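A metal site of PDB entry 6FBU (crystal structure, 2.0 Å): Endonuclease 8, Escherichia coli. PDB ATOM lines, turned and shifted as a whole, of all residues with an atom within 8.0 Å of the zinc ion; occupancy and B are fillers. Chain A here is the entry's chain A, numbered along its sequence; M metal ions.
The zinc ion is bound by SG of Cys 257 (2.1 Å), SG of Cys 237 (2.2 Å), SG of Cys 260 (2.4 Å) and SG of Cys 240 (2.5 Å).
The zinc ion has four donor atoms within binding distance.
Along chain A the residues within 4 Å of the zinc ion span positions 237 to 260.
N of Gly 259 sits close to SG of Cys 257 (3.1 Å).
The backbone NH (N) of Cys 257 lies within hydrogen-bond range of the side-chain amide oxygen (OE1) of Gln 261 (2.8 Å).
The indole nitrogen of Trp 176 sits close to the side-chain sulfur of Cys 237, 3.5 Å away.
The backbone NH (N) of Cys 237 lies within hydrogen-bond range of the backbone carbonyl oxygen (O) of Ser 242 (2.6 Å).
The backbone NH of Arg 239 lies close to the side-chain sulfur of Cys 237 (3.3 Å).
NE1 of Trp 176 lies close to SG of Cys 260 (3.6 Å).
The guanidinium group (NH2) of Arg 239 sits close to the side-chain sulfur (SG) of Cys 260.
SG of Cys 240 sits close to N of Ser 242 (3.3 Å).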
ATOM      1  N   TRP A 176     -19.385   9.289  -2.920  1.00  0.00           N
ATOM      2  CA  TRP A 176     -20.204   8.728  -3.993  1.00  0.00           C
ATOM      3  C   TRP A 176     -19.661   9.090  -5.363  1.00  0.00           C
ATOM      4  O   TRP A 176     -19.631   8.261  -6.283  1.00  0.00           O
ATOM      5  CB  TRP A 176     -21.655   9.202  -3.906  1.00  0.00           C
ATOM      6  CG  TRP A 176     -22.539   8.623  -5.032  1.00  0.00           C
ATOM      7  CD1 TRP A 176     -23.195   7.448  -5.025  1.00  0.00           C
ATOM      8  CD2 TRP A 176     -22.749   9.197  -6.327  1.00  0.00           C
ATOM      9  NE1 TRP A 176     -23.871   7.267  -6.212  1.00  0.00           N
ATOM     10  CE2 TRP A 176     -23.605   8.334  -7.035  1.00  0.00           C
ATOM     11  CE3 TRP A 176     -22.319  10.376  -6.959  1.00  0.00           C
ATOM     12  CZ2 TRP A 176     -24.019   8.595  -8.333  1.00  0.00           C
ATOM     13  CZ3 TRP A 176     -22.746  10.635  -8.250  1.00  0.00           C
ATOM     14  CH2 TRP A 176     -23.582   9.749  -8.922  1.00  0.00           C
ATOM     15  N   LYS A 228     -26.526  13.787  -4.827  1.00  0.00           N
ATOM     16  CA  LYS A 228     -26.686  12.508  -5.488  1.00  0.00           C
ATOM     17  C   LYS A 228     -27.119  11.417  -4.535  1.00  0.00           C
ATOM     18  O   LYS A 228     -27.836  10.494  -4.939  1.00  0.00           O
ATOM     19  CB  LYS A 228     -25.381  12.108  -6.179  1.00  0.00           C
ATOM     20  CG  LYS A 228     -24.828  13.150  -7.117  1.00  0.00           C
ATOM     21  CD  LYS A 228     -25.762  13.367  -8.297  1.00  0.00           C
ATOM     22  CE  LYS A 228     -25.216  14.380  -9.280  1.00  0.00           C
ATOM     23  NZ  LYS A 228     -23.859  13.969  -9.748  1.00  0.00           N
ATOM     24  N   VAL A 229     -26.725  11.506  -3.282  1.00  0.00           N
ATOM     25  CA  VAL A 229     -27.130  10.494  -2.331  1.00  0.00           C
ATOM     26  C   VAL A 229     -27.625  11.092  -1.018  1.00  0.00           C
ATOM     27  O   VAL A 229     -28.489  10.540  -0.367  1.00  0.00           O
ATOM     28  CB  VAL A 229     -26.035   9.459  -2.077  1.00  0.00           C
ATOM     29  CG1 VAL A 229     -25.560   8.885  -3.388  1.00  0.00           C
ATOM     30  CG2 VAL A 229     -24.899  10.046  -1.282  1.00  0.00           C
ATOM     31  N   GLU A 235     -34.232   6.120  -2.706  1.00  0.00           N
ATOM     32  CA  GLU A 235     -34.355   6.466  -4.109  1.00  0.00           C
ATOM     33  C   GLU A 235     -33.353   5.681  -4.949  1.00  0.00           C
ATOM     34  O   GLU A 235     -32.313   5.250  -4.451  1.00  0.00           O
ATOM     35  CB  GLU A 235     -34.114   7.964  -4.319  1.00  0.00           C
ATOM     36  CG  GLU A 235     -35.047   8.876  -3.550  1.00  0.00           C
ATOM     37  CD  GLU A 235     -34.841  10.348  -3.913  1.00  0.00           C
ATOM     38  OE1 GLU A 235     -34.934  10.678  -5.117  1.00  0.00           O
ATOM     39  OE2 GLU A 235     -34.570  11.151  -3.005  1.00  0.00           O
ATOM     40  N   PRO A 236     -33.652   5.476  -6.243  1.00  0.00           N
ATOM     41  CA  PRO A 236     -32.685   4.796  -7.109  1.00  0.00           C
ATOM     42  C   PRO A 236     -31.518   5.716  -7.430  1.00  0.00           C
ATOM     43  O   PRO A 236     -31.695   6.864  -7.839  1.00  0.00           O
ATOM     44  CB  PRO A 236     -33.496   4.461  -8.361  1.00  0.00           C
ATOM     45  CG  PRO A 236     -34.600   5.463  -8.373  1.00  0.00           C
ATOM     46  CD  PRO A 236     -34.949   5.656  -6.915  1.00  0.00           C
ATOM     47  N   CYS A 237     -30.314   5.205  -7.187  1.00  0.00           N
ATOM     48  CA  CYS A 237     -29.094   5.886  -7.581  1.00  0.00           C
ATOM     49  C   CYS A 237     -29.167   6.306  -9.033  1.00  0.00           C
ATOM     50  O   CYS A 237     -29.574   5.522  -9.896  1.00  0.00           O
ATOM     51  CB  CYS A 237     -27.902   4.946  -7.350  1.00  0.00           C
ATOM     52  SG  CYS A 237     -26.305   5.493  -7.985  1.00  0.00           S
ATOM     53  N   GLU A 238     -28.796   7.553  -9.317  1.00  0.00           N
ATOM     54  CA  GLU A 238     -28.864   7.990 -10.705  1.00  0.00           C
ATOM     55  C   GLU A 238     -27.738   7.433 -11.569  1.00  0.00           C
ATOM     56  O   GLU A 238     -27.816   7.541 -12.794  1.00  0.00           O
ATOM     57  CB  GLU A 238     -28.914   9.520 -10.776  1.00  0.00           C
ATOM     58  CG  GLU A 238     -27.724  10.258 -10.215  1.00  0.00           C
ATOM     59  CD  GLU A 238     -27.928  11.759 -10.283  1.00  0.00           C
ATOM     60  OE1 GLU A 238     -28.623  12.300  -9.387  1.00  0.00           O
ATOM     61  OE2 GLU A 238     -27.402  12.396 -11.211  1.00  0.00           O
ATOM     62  N   ARG A 239     -26.715   6.846 -10.967  1.00  0.00           N
ATOM     63  CA  ARG A 239     -25.632   6.244 -11.737  1.00  0.00           C
ATOM     64  C   ARG A 239     -25.876   4.766 -12.016  1.00  0.00           C
ATOM     65  O   ARG A 239     -25.676   4.301 -13.145  1.00  0.00           O
ATOM     66  CB  ARG A 239     -24.298   6.416 -10.995  1.00  0.00           C
ATOM     67  CG  ARG A 239     -23.111   5.754 -11.687  1.00  0.00           C
ATOM     68  CD  ARG A 239     -21.740   6.347 -11.239  1.00  0.00           C
ATOM     69  NE  ARG A 239     -21.479   6.044  -9.847  1.00  0.00           N
ATOM     70  CZ  ARG A 239     -20.819   6.823  -9.002  1.00  0.00           C
ATOM     71  NH1 ARG A 239     -20.300   7.988  -9.408  1.00  0.00           N
ATOM     72  NH2 ARG A 239     -20.666   6.401  -7.755  1.00  0.00           N
ATOM     73  N   CYS A 240     -26.345   4.009 -11.030  1.00  0.00           N
ATOM     74  CA  CYS A 240     -26.448   2.573 -11.210  1.00  0.00           C
ATOM     75  C   CYS A 240     -27.826   1.989 -10.918  1.00  0.00           C
ATOM     76  O   CYS A 240     -27.987   0.770 -11.038  1.00  0.00           O
ATOM     77  CB  CYS A 240     -25.409   1.862 -10.327  1.00  0.00           C
ATOM     78  SG  CYS A 240     -26.023   1.561  -8.684  1.00  0.00           S
ATOM     79  N   GLY A 241     -28.805   2.803 -10.535  1.00  0.00           N
ATOM     80  CA  GLY A 241     -30.145   2.307 -10.279  1.00  0.00           C
ATOM     81  C   GLY A 241     -30.357   1.675  -8.928  1.00  0.00           C
ATOM     82  O   GLY A 241     -31.507   1.504  -8.516  1.00  0.00           O
ATOM     83  N   SER A 242     -29.297   1.312  -8.211  1.00  0.00           N
ATOM     84  CA  SER A 242     -29.484   0.683  -6.913  1.00  0.00           C
ATOM     85  C   SER A 242     -30.099   1.681  -5.919  1.00  0.00           C
ATOM     86  O   SER A 242     -30.086   2.899  -6.121  1.00  0.00           O
ATOM     87  CB  SER A 242     -28.159   0.151  -6.396  1.00  0.00           C
ATOM     88  OG  SER A 242     -27.775  -1.017  -7.121  1.00  0.00           O
ATOM     89  N   ILE A 243     -30.661   1.137  -4.851  1.00  0.00           N
ATOM     90  CA  ILE A 243     -31.438   1.933  -3.898  1.00  0.00           C
ATOM     91  C   ILE A 243     -30.486   2.499  -2.854  1.00  0.00           C
ATOM     92  O   ILE A 243     -29.803   1.739  -2.153  1.00  0.00           O
ATOM     93  CB  ILE A 243     -32.552   1.095  -3.261  1.00  0.00           C
ATOM     94  CG1 ILE A 243     -33.607   0.707  -4.313  1.00  0.00           C
ATOM     95  CG2 ILE A 243     -33.188   1.853  -2.099  1.00  0.00           C
ATOM     96  CD1 ILE A 243     -34.124   1.875  -5.165  1.00  0.00           C
ATOM     97  N   ILE A 244     -30.446   3.824  -2.761  1.00  0.00           N
ATOM     98  CA  ILE A 244     -29.519   4.494  -1.847  1.00  0.00           C
ATOM     99  C   ILE A 244     -29.914   4.214  -0.412  1.00  0.00           C
ATOM    100  O   ILE A 244     -31.102   4.196  -0.072  1.00  0.00           O
ATOM    101  CB  ILE A 244     -29.494   6.005  -2.150  1.00  0.00           C
ATOM    102  CG1 ILE A 244     -28.835   6.257  -3.501  1.00  0.00           C
ATOM    103  CG2 ILE A 244     -28.794   6.769  -1.024  1.00  0.00           C
ATOM    104  CD1 ILE A 244     -29.470   7.401  -4.263  1.00  0.00           C
ATOM    105  N   TRP A 256     -25.276   6.435   0.929  1.00  0.00           N
ATOM    106  CA  TRP A 256     -24.441   5.814  -0.073  1.00  0.00           C
ATOM    107  C   TRP A 256     -25.204   4.820  -0.937  1.00  0.00           C
ATOM    108  O   TRP A 256     -26.271   4.352  -0.565  1.00  0.00           O
ATOM    109  CB  TRP A 256     -23.187   5.210   0.553  1.00  0.00           C
ATOM    110  CG  TRP A 256     -23.260   3.766   0.877  1.00  0.00           C
ATOM    111  CD1 TRP A 256     -22.655   2.746   0.232  1.00  0.00           C
ATOM    112  CD2 TRP A 256     -24.007   3.173   1.936  1.00  0.00           C
ATOM    113  NE1 TRP A 256     -22.953   1.561   0.817  1.00  0.00           N
ATOM    114  CE2 TRP A 256     -23.787   1.798   1.878  1.00  0.00           C
ATOM    115  CE3 TRP A 256     -24.833   3.680   2.935  1.00  0.00           C
ATOM    116  CZ2 TRP A 256     -24.365   0.924   2.756  1.00  0.00           C
ATOM    117  CZ3 TRP A 256     -25.395   2.812   3.814  1.00  0.00           C
ATOM    118  CH2 TRP A 256     -25.165   1.447   3.720  1.00  0.00           C
ATOM    119  N   CYS A 257     -24.642   4.493  -2.087  1.00  0.00           N
ATOM    120  CA  CYS A 257     -25.286   3.545  -2.952  1.00  0.00           C
ATOM    121  C   CYS A 257     -24.499   2.253  -2.914  1.00  0.00           C
ATOM    122  O   CYS A 257     -23.328   2.232  -3.264  1.00  0.00           O
ATOM    123  CB  CYS A 257     -25.366   4.053  -4.378  1.00  0.00           C
ATOM    124  SG  CYS A 257     -25.880   2.790  -5.572  1.00  0.00           S
ATOM    125  N   PRO A 258     -25.130   1.177  -2.460  1.00  0.00           N
ATOM    126  CA  PRO A 258     -24.430  -0.109  -2.436  1.00  0.00           C
ATOM    127  C   PRO A 258     -24.046  -0.587  -3.825  1.00  0.00           C
ATOM    128  O   PRO A 258     -23.133  -1.412  -3.955  1.00  0.00           O
ATOM    129  CB  PRO A 258     -25.448  -1.049  -1.784  1.00  0.00           C
ATOM    130  CG  PRO A 258     -26.789  -0.492  -2.241  1.00  0.00           C
ATOM    131  CD  PRO A 258     -26.595   1.015  -2.416  1.00  0.00           C
ATOM    132  N   GLY A 259     -24.678  -0.035  -4.869  1.00  0.00           N
ATOM    133  CA  GLY A 259     -24.483  -0.572  -6.210  1.00  0.00           C
ATOM    134  C   GLY A 259     -23.224  -0.103  -6.890  1.00  0.00           C
ATOM    135  O   GLY A 259     -22.695  -0.806  -7.755  1.00  0.00           O
ATOM    136  N   CYS A 260     -22.715   1.069  -6.504  1.00  0.00           N
ATOM    137  CA  CYS A 260     -21.554   1.612  -7.184  1.00  0.00           C
ATOM    138  C   CYS A 260     -20.544   2.286  -6.246  1.00  0.00           C
ATOM    139  O   CYS A 260     -19.693   3.056  -6.715  1.00  0.00           O
ATOM    140  CB  CYS A 260     -21.975   2.622  -8.244  1.00  0.00           C
ATOM    141  SG  CYS A 260     -22.893   4.018  -7.550  1.00  0.00           S
ATOM    142  N   GLN A 261     -20.616   2.036  -4.934  1.00  0.00           N
ATOM    143  CA  GLN A 261     -19.609   2.504  -3.989  1.00  0.00           C
ATOM    144  C   GLN A 261     -18.972   1.291  -3.320  1.00  0.00           C
ATOM    145  O   GLN A 261     -19.677   0.506  -2.681  1.00  0.00           O
ATOM    146  CB  GLN A 261     -20.203   3.454  -2.936  1.00  0.00           C
ATOM    147  CG  GLN A 261     -20.458   4.857  -3.451  1.00  0.00           C
ATOM    148  CD  GLN A 261     -21.086   5.763  -2.409  1.00  0.00           C
ATOM    149  OE1 GLN A 261     -22.290   6.003  -2.420  1.00  0.00           O
ATOM    150  NE2 GLN A 261     -20.256   6.251  -1.482  1.00  0.00           N
ATOM    151  N   HIS A 262     -17.659   1.157  -3.455  1.00  0.00           N
ATOM    152  CA  HIS A 262     -16.969  -0.051  -3.017  1.00  0.00           C
ATOM    153  C   HIS A 262     -15.684   0.246  -2.265  1.00  0.00           C
ATOM    154  O   HIS A 262     -15.319   1.416  -2.091  1.00  0.00           O
ATOM    155  CB  HIS A 262     -16.675  -0.927  -4.227  1.00  0.00           C
ATOM    156  CG  HIS A 262     -17.873  -1.166  -5.078  1.00  0.00           C
ATOM    157  ND1 HIS A 262     -18.851  -2.088  -4.741  1.00  0.00           N
ATOM    158  CD2 HIS A 262     -18.294  -0.577  -6.222  1.00  0.00           C
ATOM    159  CE1 HIS A 262     -19.788  -2.082  -5.665  1.00  0.00           C
ATOM    160  NE2 HIS A 262     -19.477  -1.173  -6.566  1.00  0.00           N
ATOM    161  OXT HIS A 262     -15.001  -0.670  -1.816  1.00  0.00           O
HETATM  162 ZN    ZN M   1     -25.263   3.588  -7.463  1.00  0.00          ZN
